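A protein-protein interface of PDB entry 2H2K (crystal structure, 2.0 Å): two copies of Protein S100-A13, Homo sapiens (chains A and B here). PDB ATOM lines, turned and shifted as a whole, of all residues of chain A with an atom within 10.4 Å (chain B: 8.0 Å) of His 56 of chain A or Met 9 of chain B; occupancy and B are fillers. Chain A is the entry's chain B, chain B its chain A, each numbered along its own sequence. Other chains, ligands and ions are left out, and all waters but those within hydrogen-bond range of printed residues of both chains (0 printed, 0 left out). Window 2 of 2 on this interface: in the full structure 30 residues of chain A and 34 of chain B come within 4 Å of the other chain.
O of Gln 52 of chain A touches CG2 of Thr 15 of chain B, 3.6 Å away.
O of Gln 53 of chain A touches CG of Glu 18 of chain B (3.3 Å).
C of Leu 54 of chain A touches OE2 of Glu 18 of chain B, 3.3 Å away.
CB of Pro 55 of chain A touches CE of Met 9 of chain B (3.9 Å).
Pro 55 of chain A touches Thr 15 of chain B.
Met 9 of chain B touches His 56 of chain A (O to CE1, 3.0 Å).
O of Glu 12 of chain B touches CE1 of His 56 of chain A, at 3.2 Å.
His 56 of chain A touches Pro 13 of chain B.
His 56 of chain A touches Leu 14 of chain B (CG to CD2, 3.9 Å).
No position is printed for both chains.
Of the 13 pairs that touch across the chains among the printed residues, none has its exchanged pair printed and touching as well.
The side-chain carboxylate (OE1) of Glu 18 of chain B lies within hydrogen-bond range of the backbone NH (N) of Thr 15 of chain B, 3.1 Å away.
The side-chain hydroxyl (OG) of Ser 7 of chain B sits close to the backbone NH (N) of Met 9 of chain B.
Of the 18 printed residues of chain A, 6 touch a printed residue of chain B.
Hydrophobic or aromatic side chains of chain B within 4 Å of the printed part of chain A: Met 9 and Leu 14.
Along chain B the printed residues that touch a printed residue of chain A span positions 9 to 18.
Among the printed residues, no Asp or Glu carboxylate lies within 4 Å of a Lys or Arg side-chain nitrogen of the other chain.
Of chain B, only Met 9, Glu 12, Pro 13, Leu 14 and Glu 18 come within 4 Å of His 56 of chain A.
Met 9 of chain B touches just these residues of chain A: Pro 55 (3.9 Å) and His 56 (3.0 Å).
No residue of chain A comes within 4 Å of Ser 7 of chain B.
No residue of chain A comes within 4 Å of Ala 11 of chain B.
Glu 12 of chain B touches one residue of chain A.
Of the printed residues of chain A, Pro 13 of chain B touches His 56.
Of the printed residues of chain A, Glu 18 of chain B touches Gln 53 (3.3 Å), Leu 54 (3.3 Å), Pro 55 (3.3 Å), His 56 (2.7 Å) and Leu 57 (3.0 Å).
Val 61 of chain A touches none of the printed residues of chain B.
The nearest residue of chain B that does not touch His 56 of chain A is Thr 15 of chain B (4.7 Å).
The nearest residue of chain A that does not touch Met 9 of chain B is Lys 59 of chain A (4.8 Å).
OE2 of Glu 18 of chain B sits at hydrogen-bond distance from N of Leu 57 of chain A.
The side-chain carboxylate (OE2) of Glu 18 of chain B sits close to the backbone nitrogen (N) of Pro 55 of chain A, at 3.3 Å.
The side-chain carboxylate (OE2) of Glu 18 of chain B sits at hydrogen-bond distance from the backbone NH (N) of His 56 of chain A, at 2.7 Å.
The side-chain hydroxyl (OG1) of Thr 15 of chain B lies within hydrogen-bond range of the backbone carbonyl oxygen (O) of Gln 53 of chain A (2.6 Å).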
ATOM      1  N   LEU A  49     -26.767 -19.461  34.899  1.00  0.00           N
ATOM      2  CA  LEU A  49     -28.007 -18.893  34.393  1.00  0.00           C
ATOM      3  C   LEU A  49     -27.645 -17.598  33.666  1.00  0.00           C
ATOM      4  O   LEU A  49     -28.069 -17.374  32.531  1.00  0.00           O
ATOM      5  CB  LEU A  49     -28.990 -18.620  35.538  1.00  0.00           C
ATOM      6  CG  LEU A  49     -30.387 -18.197  35.064  1.00  0.00           C
ATOM      7  CD1 LEU A  49     -31.439 -18.611  36.077  1.00  0.00           C
ATOM      8  CD2 LEU A  49     -30.400 -16.709  34.816  1.00  0.00           C
ATOM      9  N   VAL A  50     -26.835 -16.760  34.304  1.00  0.00           N
ATOM     10  CA  VAL A  50     -26.414 -15.498  33.698  1.00  0.00           C
ATOM     11  C   VAL A  50     -25.699 -15.682  32.359  1.00  0.00           C
ATOM     12  O   VAL A  50     -26.162 -15.208  31.326  1.00  0.00           O
ATOM     13  CB  VAL A  50     -25.471 -14.695  34.637  1.00  0.00           C
ATOM     14  CG1 VAL A  50     -24.861 -13.511  33.880  1.00  0.00           C
ATOM     15  CG2 VAL A  50     -26.242 -14.184  35.845  1.00  0.00           C
ATOM     16  N   THR A  51     -24.574 -16.384  32.376  1.00  0.00           N
ATOM     17  CA  THR A  51     -23.796 -16.574  31.157  1.00  0.00           C
ATOM     18  C   THR A  51     -24.528 -17.336  30.056  1.00  0.00           C
ATOM     19  O   THR A  51     -24.232 -17.157  28.877  1.00  0.00           O
ATOM     20  CB  THR A  51     -22.433 -17.253  31.458  1.00  0.00           C
ATOM     21  OG1 THR A  51     -22.641 -18.507  32.110  1.00  0.00           O
ATOM     22  CG2 THR A  51     -21.598 -16.363  32.366  1.00  0.00           C
ATOM     23  N   GLN A  52     -25.478 -18.179  30.448  1.00  0.00           N
ATOM     24  CA  GLN A  52     -26.214 -19.001  29.494  1.00  0.00           C
ATOM     25  C   GLN A  52     -27.410 -18.245  28.923  1.00  0.00           C
ATOM     26  O   GLN A  52     -27.699 -18.332  27.730  1.00  0.00           O
ATOM     27  CB  GLN A  52     -26.679 -20.301  30.154  1.00  0.00           C
ATOM     28  CG  GLN A  52     -25.653 -21.421  30.108  1.00  0.00           C
ATOM     29  CD  GLN A  52     -26.276 -22.791  30.295  1.00  0.00           C
ATOM     30  OE1 GLN A  52     -27.340 -23.074  29.744  1.00  0.00           O
ATOM     31  NE2 GLN A  52     -25.617 -23.642  31.072  1.00  0.00           N
ATOM     32  N   GLN A  53     -28.101 -17.505  29.783  1.00  0.00           N
ATOM     33  CA  GLN A  53     -29.465 -17.075  29.501  1.00  0.00           C
ATOM     34  C   GLN A  53     -29.594 -15.558  29.582  1.00  0.00           C
ATOM     35  O   GLN A  53     -30.639 -14.996  29.258  1.00  0.00           O
ATOM     36  CB  GLN A  53     -30.448 -17.739  30.468  1.00  0.00           C
ATOM     37  CG  GLN A  53     -30.998 -19.069  29.980  1.00  0.00           C
ATOM     38  CD  GLN A  53     -31.648 -18.964  28.614  1.00  0.00           C
ATOM     39  OE1 GLN A  53     -31.273 -19.681  27.687  1.00  0.00           O
ATOM     40  NE2 GLN A  53     -32.622 -18.070  28.487  1.00  0.00           N
ATOM     41  N   LEU A  54     -28.524 -14.901  30.018  1.00  0.00           N
ATOM     42  CA  LEU A  54     -28.531 -13.453  30.188  1.00  0.00           C
ATOM     43  C   LEU A  54     -27.239 -12.831  29.670  1.00  0.00           C
ATOM     44  O   LEU A  54     -26.732 -11.863  30.238  1.00  0.00           O
ATOM     45  CB  LEU A  54     -28.736 -13.088  31.660  1.00  0.00           C
ATOM     46  CG  LEU A  54     -30.120 -13.378  32.242  1.00  0.00           C
ATOM     47  CD1 LEU A  54     -30.160 -13.046  33.727  1.00  0.00           C
ATOM     48  CD2 LEU A  54     -31.193 -12.606  31.489  1.00  0.00           C
ATOM     49  N   PRO A  55     -26.710 -13.392  28.587  1.00  0.00           N
ATOM     50  CA  PRO A  55     -25.435 -12.932  28.023  1.00  0.00           C
ATOM     51  C   PRO A  55     -25.468 -11.521  27.441  1.00  0.00           C
ATOM     52  O   PRO A  55     -24.439 -10.857  27.374  1.00  0.00           O
ATOM     53  CB  PRO A  55     -25.120 -13.984  26.954  1.00  0.00           C
ATOM     54  CG  PRO A  55     -25.976 -15.174  27.346  1.00  0.00           C
ATOM     55  CD  PRO A  55     -27.242 -14.512  27.795  1.00  0.00           C
ATOM     56  N   HIS A  56     -26.641 -11.068  27.007  1.00  0.00           N
ATOM     57  CA  HIS A  56     -26.763  -9.720  26.452  1.00  0.00           C
ATOM     58  C   HIS A  56     -27.077  -8.742  27.581  1.00  0.00           C
ATOM     59  O   HIS A  56     -26.318  -7.809  27.851  1.00  0.00           O
ATOM     60  CB  HIS A  56     -27.910  -9.627  25.437  1.00  0.00           C
ATOM     61  CG  HIS A  56     -27.750 -10.489  24.222  1.00  0.00           C
ATOM     62  ND1 HIS A  56     -27.454  -9.972  22.978  1.00  0.00           N
ATOM     63  CD2 HIS A  56     -27.946 -11.817  24.041  1.00  0.00           C
ATOM     64  CE1 HIS A  56     -27.483 -10.942  22.082  1.00  0.00           C
ATOM     65  NE2 HIS A  56     -27.781 -12.072  22.701  1.00  0.00           N
ATOM     66  N   LEU A  57     -28.211  -8.975  28.241  1.00  0.00           N
ATOM     67  CA  LEU A  57     -28.668  -8.110  29.318  1.00  0.00           C
ATOM     68  C   LEU A  57     -27.666  -7.924  30.441  1.00  0.00           C
ATOM     69  O   LEU A  57     -27.666  -6.893  31.106  1.00  0.00           O
ATOM     70  CB  LEU A  57     -30.000  -8.621  29.878  1.00  0.00           C
ATOM     71  CG  LEU A  57     -31.182  -8.556  28.904  1.00  0.00           C
ATOM     72  CD1 LEU A  57     -32.470  -8.860  29.647  1.00  0.00           C
ATOM     73  CD2 LEU A  57     -31.257  -7.171  28.264  1.00  0.00           C
ATOM     74  N   LEU A  58     -26.814  -8.918  30.665  1.00  0.00           N
ATOM     75  CA  LEU A  58     -25.807  -8.787  31.708  1.00  0.00           C
ATOM     76  C   LEU A  58     -24.415  -8.781  31.107  1.00  0.00           C
ATOM     77  O   LEU A  58     -23.447  -9.163  31.763  1.00  0.00           O
ATOM     78  CB  LEU A  58     -25.935  -9.914  32.737  1.00  0.00           C
ATOM     79  CG  LEU A  58     -27.159  -9.818  33.650  1.00  0.00           C
ATOM     80  CD1 LEU A  58     -27.094 -10.903  34.717  1.00  0.00           C
ATOM     81  CD2 LEU A  58     -27.206  -8.444  34.297  1.00  0.00           C
ATOM     82  N   LYS A  59     -24.310  -8.336  29.859  1.00  0.00           N
ATOM     83  CA  LYS A  59     -23.011  -8.293  29.204  1.00  0.00           C
ATOM     84  C   LYS A  59     -22.038  -7.366  29.926  1.00  0.00           C
ATOM     85  O   LYS A  59     -20.841  -7.646  29.979  1.00  0.00           O
ATOM     86  CB  LYS A  59     -23.128  -7.845  27.738  1.00  0.00           C
ATOM     87  CG  LYS A  59     -21.753  -7.768  27.066  1.00  0.00           C
ATOM     88  CD  LYS A  59     -21.762  -7.324  25.614  1.00  0.00           C
ATOM     89  CE  LYS A  59     -20.328  -7.000  25.188  1.00  0.00           C
ATOM     90  NZ  LYS A  59     -20.143  -6.851  23.720  1.00  0.00           N
ATOM     91  N   ASP A  60     -22.555  -6.271  30.474  1.00  0.00           N
ATOM     92  CA  ASP A  60     -21.712  -5.241  31.068  1.00  0.00           C
ATOM     93  C   ASP A  60     -21.725  -5.328  32.591  1.00  0.00           C
ATOM     94  O   ASP A  60     -21.360  -4.375  33.279  1.00  0.00           O
ATOM     95  CB  ASP A  60     -22.167  -3.851  30.617  1.00  0.00           C
ATOM     96  CG  ASP A  60     -21.852  -3.581  29.159  1.00  0.00           C
ATOM     97  OD1 ASP A  60     -20.701  -3.828  28.742  1.00  0.00           O
ATOM     98  OD2 ASP A  60     -22.690  -3.122  28.355  1.00  0.00           O
ATOM     99  N   VAL A  61     -22.148  -6.476  33.109  1.00  0.00           N
ATOM    100  CA  VAL A  61     -22.037  -6.759  34.536  1.00  0.00           C
ATOM    101  C   VAL A  61     -20.605  -7.115  34.917  1.00  0.00           C
ATOM    102  O   VAL A  61     -19.887  -7.753  34.147  1.00  0.00           O
ATOM    103  CB  VAL A  61     -22.972  -7.908  34.957  1.00  0.00           C
ATOM    104  CG1 VAL A  61     -22.268  -9.248  34.811  1.00  0.00           C
ATOM    105  CG2 VAL A  61     -23.456  -7.704  36.384  1.00  0.00           C
ATOM    106  N   GLY A  62     -20.196  -6.700  36.111  1.00  0.00           N
ATOM    107  CA  GLY A  62     -18.837  -6.921  36.571  1.00  0.00           C
ATOM    108  C   GLY A  62     -18.581  -8.366  36.951  1.00  0.00           C
ATOM    109  O   GLY A  62     -19.001  -9.286  36.249  1.00  0.00           O
ATOM    110  N   LEU A  91     -33.574  -5.807  35.401  1.00  0.00           N
ATOM    111  CA  LEU A  91     -33.411  -5.908  33.962  1.00  0.00           C
ATOM    112  C   LEU A  91     -34.625  -5.318  33.246  1.00  0.00           C
ATOM    113  O   LEU A  91     -34.481  -4.600  32.259  1.00  0.00           O
ATOM    114  CB  LEU A  91     -33.205  -7.373  33.578  1.00  0.00           C
ATOM    115  CG  LEU A  91     -31.936  -7.960  34.214  1.00  0.00           C
ATOM    116  CD1 LEU A  91     -31.815  -9.443  33.913  1.00  0.00           C
ATOM    117  CD2 LEU A  91     -30.715  -7.205  33.690  1.00  0.00           C
ATOM    118  N   GLU A  94     -34.508  -1.468  33.094  1.00  0.00           N
ATOM    119  CA  GLU A  94     -33.575  -0.940  32.109  1.00  0.00           C
ATOM    120  C   GLU A  94     -34.167  -1.007  30.711  1.00  0.00           C
ATOM    121  O   GLU A  94     -34.009  -0.080  29.912  1.00  0.00           O
ATOM    122  CB  GLU A  94     -32.255  -1.706  32.171  1.00  0.00           C
ATOM    123  CG  GLU A  94     -31.493  -1.435  33.448  1.00  0.00           C
ATOM    124  CD  GLU A  94     -31.334   0.055  33.690  1.00  0.00           C
ATOM    125  OE1 GLU A  94     -30.755   0.733  32.820  1.00  0.00           O
ATOM    126  OE2 GLU A  94     -31.792   0.550  34.743  1.00  0.00           O
ATOM    127  N   ILE A  95     -34.850  -2.106  30.415  1.00  0.00           N
ATOM    128  CA  ILE A  95     -35.485  -2.255  29.112  1.00  0.00           C
ATOM    129  C   ILE A  95     -36.588  -1.212  28.997  1.00  0.00           C
ATOM    130  O   ILE A  95     -36.794  -0.625  27.934  1.00  0.00           O
ATOM    131  CB  ILE A  95     -36.099  -3.654  28.953  1.00  0.00           C
ATOM    132  CG1 ILE A  95     -34.985  -4.702  28.901  1.00  0.00           C
ATOM    133  CG2 ILE A  95     -36.965  -3.714  27.704  1.00  0.00           C
ATOM    134  CD1 ILE A  95     -35.500  -6.124  29.010  1.00  0.00           C
ATOM    135  N   LYS A  98     -35.506   2.080  27.756  1.00  0.00           N
ATOM    136  CA  LYS A  98     -35.241   2.091  26.319  1.00  0.00           C
ATOM    137  C   LYS A  98     -36.519   2.111  25.478  1.00  0.00           C
ATOM    138  O   LYS A  98     -36.557   2.729  24.413  1.00  0.00           O
ATOM    139  CB  LYS A  98     -34.413   0.865  25.904  1.00  0.00           C
ATOM    140  CG  LYS A  98     -32.997   0.767  26.464  1.00  0.00           C
ATOM    141  CD  LYS A  98     -32.264  -0.388  25.761  1.00  0.00           C
ATOM    142  CE  LYS A  98     -31.075  -0.900  26.568  1.00  0.00           C
ATOM    143  NZ  LYS A  98     -31.092  -2.398  26.704  1.00  0.00           N
ATOM    144  N   SER B   7     -21.025  -5.353  16.176  1.00  0.00           N
ATOM    145  CA  SER B   7     -20.914  -6.210  17.391  1.00  0.00           C
ATOM    146  C   SER B   7     -21.333  -7.644  17.100  1.00  0.00           C
ATOM    147  O   SER B   7     -22.395  -7.881  16.524  1.00  0.00           O
ATOM    148  CB  SER B   7     -21.782  -5.640  18.517  1.00  0.00           C
ATOM    149  OG  SER B   7     -22.138  -6.650  19.449  1.00  0.00           O
ATOM    150  N   LEU B   8     -20.503  -8.600  17.511  1.00  0.00           N
ATOM    151  CA  LEU B   8     -20.817 -10.005  17.283  1.00  0.00           C
ATOM    152  C   LEU B   8     -22.055 -10.426  18.072  1.00  0.00           C
ATOM    153  O   LEU B   8     -22.928 -11.107  17.537  1.00  0.00           O
ATOM    154  CB  LEU B   8     -19.619 -10.893  17.654  1.00  0.00           C
ATOM    155  CG  LEU B   8     -18.290 -10.622  16.935  1.00  0.00           C
ATOM    156  CD1 LEU B   8     -17.273 -11.686  17.337  1.00  0.00           C
ATOM    157  CD2 LEU B   8     -18.490 -10.631  15.425  1.00  0.00           C
ATOM    158  N   MET B   9     -22.143 -10.015  19.335  1.00  0.00           N
ATOM    159  CA  MET B   9     -23.302 -10.373  20.152  1.00  0.00           C
ATOM    160  C   MET B   9     -24.586  -9.741  19.615  1.00  0.00           C
ATOM    161  O   MET B   9     -25.676 -10.257  19.849  1.00  0.00           O
ATOM    162  CB  MET B   9     -23.121  -9.947  21.615  1.00  0.00           C
ATOM    163  CG  MET B   9     -22.327 -10.926  22.486  1.00  0.00           C
ATOM    164  SD  MET B   9     -22.767 -12.682  22.281  1.00  0.00           S
ATOM    165  CE  MET B   9     -24.245 -12.841  23.296  1.00  0.00           C
ATOM    166  N   ALA B  10     -24.459  -8.629  18.896  1.00  0.00           N
ATOM    167  CA  ALA B  10     -25.629  -7.959  18.341  1.00  0.00           C
ATOM    168  C   ALA B  10     -26.322  -8.839  17.303  1.00  0.00           C
ATOM    169  O   ALA B  10     -27.529  -8.734  17.099  1.00  0.00           O
ATOM    170  CB  ALA B  10     -25.222  -6.628  17.715  1.00  0.00           C
ATOM    171  N   ALA B  11     -25.555  -9.711  16.657  1.00  0.00           N
ATOM    172  CA  ALA B  11     -26.099 -10.606  15.638  1.00  0.00           C
ATOM    173  C   ALA B  11     -26.594 -11.920  16.234  1.00  0.00           C
ATOM    174  O   ALA B  11     -27.079 -12.796  15.515  1.00  0.00           O
ATOM    175  CB  ALA B  11     -25.049 -10.884  14.569  1.00  0.00           C
ATOM    176  N   GLU B  12     -26.448 -12.065  17.547  1.00  0.00           N
ATOM    177  CA  GLU B  12     -26.912 -13.265  18.229  1.00  0.00           C
ATOM    178  C   GLU B  12     -28.335 -12.970  18.672  1.00  0.00           C
ATOM    179  O   GLU B  12     -28.614 -11.898  19.206  1.00  0.00           O
ATOM    180  CB  GLU B  12     -26.046 -13.577  19.455  1.00  0.00           C
ATOM    181  CG  GLU B  12     -24.822 -14.447  19.177  1.00  0.00           C
ATOM    182  CD  GLU B  12     -25.189 -15.853  18.729  1.00  0.00           C
ATOM    183  OE1 GLU B  12     -26.358 -16.254  18.914  1.00  0.00           O
ATOM    184  OE2 GLU B  12     -24.301 -16.560  18.200  1.00  0.00           O
ATOM    185  N   PRO B  13     -29.258 -13.914  18.448  1.00  0.00           N
ATOM    186  CA  PRO B  13     -30.641 -13.672  18.860  1.00  0.00           C
ATOM    187  C   PRO B  13     -30.781 -13.731  20.378  1.00  0.00           C
ATOM    188  O   PRO B  13     -30.033 -14.439  21.054  1.00  0.00           O
ATOM    189  CB  PRO B  13     -31.404 -14.775  18.140  1.00  0.00           C
ATOM    190  CG  PRO B  13     -30.435 -15.915  18.166  1.00  0.00           C
ATOM    191  CD  PRO B  13     -29.110 -15.248  17.835  1.00  0.00           C
ATOM    192  N   LEU B  14     -31.728 -12.966  20.912  1.00  0.00           N
ATOM    193  CA  LEU B  14     -31.952 -12.933  22.350  1.00  0.00           C
ATOM    194  C   LEU B  14     -32.222 -14.323  22.867  1.00  0.00           C
ATOM    195  O   LEU B  14     -32.785 -15.158  22.160  1.00  0.00           O
ATOM    196  CB  LEU B  14     -33.142 -12.042  22.697  1.00  0.00           C
ATOM    197  CG  LEU B  14     -32.867 -10.546  22.601  1.00  0.00           C
ATOM    198  CD1 LEU B  14     -34.032  -9.776  23.214  1.00  0.00           C
ATOM    199  CD2 LEU B  14     -31.572 -10.220  23.334  1.00  0.00           C
ATOM    200  N   THR B  15     -31.799 -14.591  24.097  1.00  0.00           N
ATOM    201  CA  THR B  15     -32.065 -15.898  24.646  1.00  0.00           C
ATOM    202  C   THR B  15     -33.546 -15.914  24.911  1.00  0.00           C
ATOM    203  O   THR B  15     -34.235 -14.894  24.819  1.00  0.00           O
ATOM    204  CB  THR B  15     -31.343 -16.159  25.978  1.00  0.00           C
ATOM    205  OG1 THR B  15     -31.742 -15.178  26.943  1.00  0.00           O
ATOM    206  CG2 THR B  15     -29.841 -16.121  25.779  1.00  0.00           C
ATOM    207  N   GLU B  18     -34.255 -13.551  27.958  1.00  0.00           N
ATOM    208  CA  GLU B  18     -34.156 -12.128  27.641  1.00  0.00           C
ATOM    209  C   GLU B  18     -35.341 -11.666  26.794  1.00  0.00           C
ATOM    210  O   GLU B  18     -35.884 -10.582  27.000  1.00  0.00           O
ATOM    211  CB  GLU B  18     -32.843 -11.845  26.900  1.00  0.00           C
ATOM    212  CG  GLU B  18     -31.595 -12.199  27.701  1.00  0.00           C
ATOM    213  CD  GLU B  18     -30.317 -12.057  26.891  1.00  0.00           C
ATOM    214  OE1 GLU B  18     -30.336 -12.415  25.699  1.00  0.00           O
ATOM    215  OE2 GLU B  18     -29.296 -11.603  27.450  1.00  0.00           O
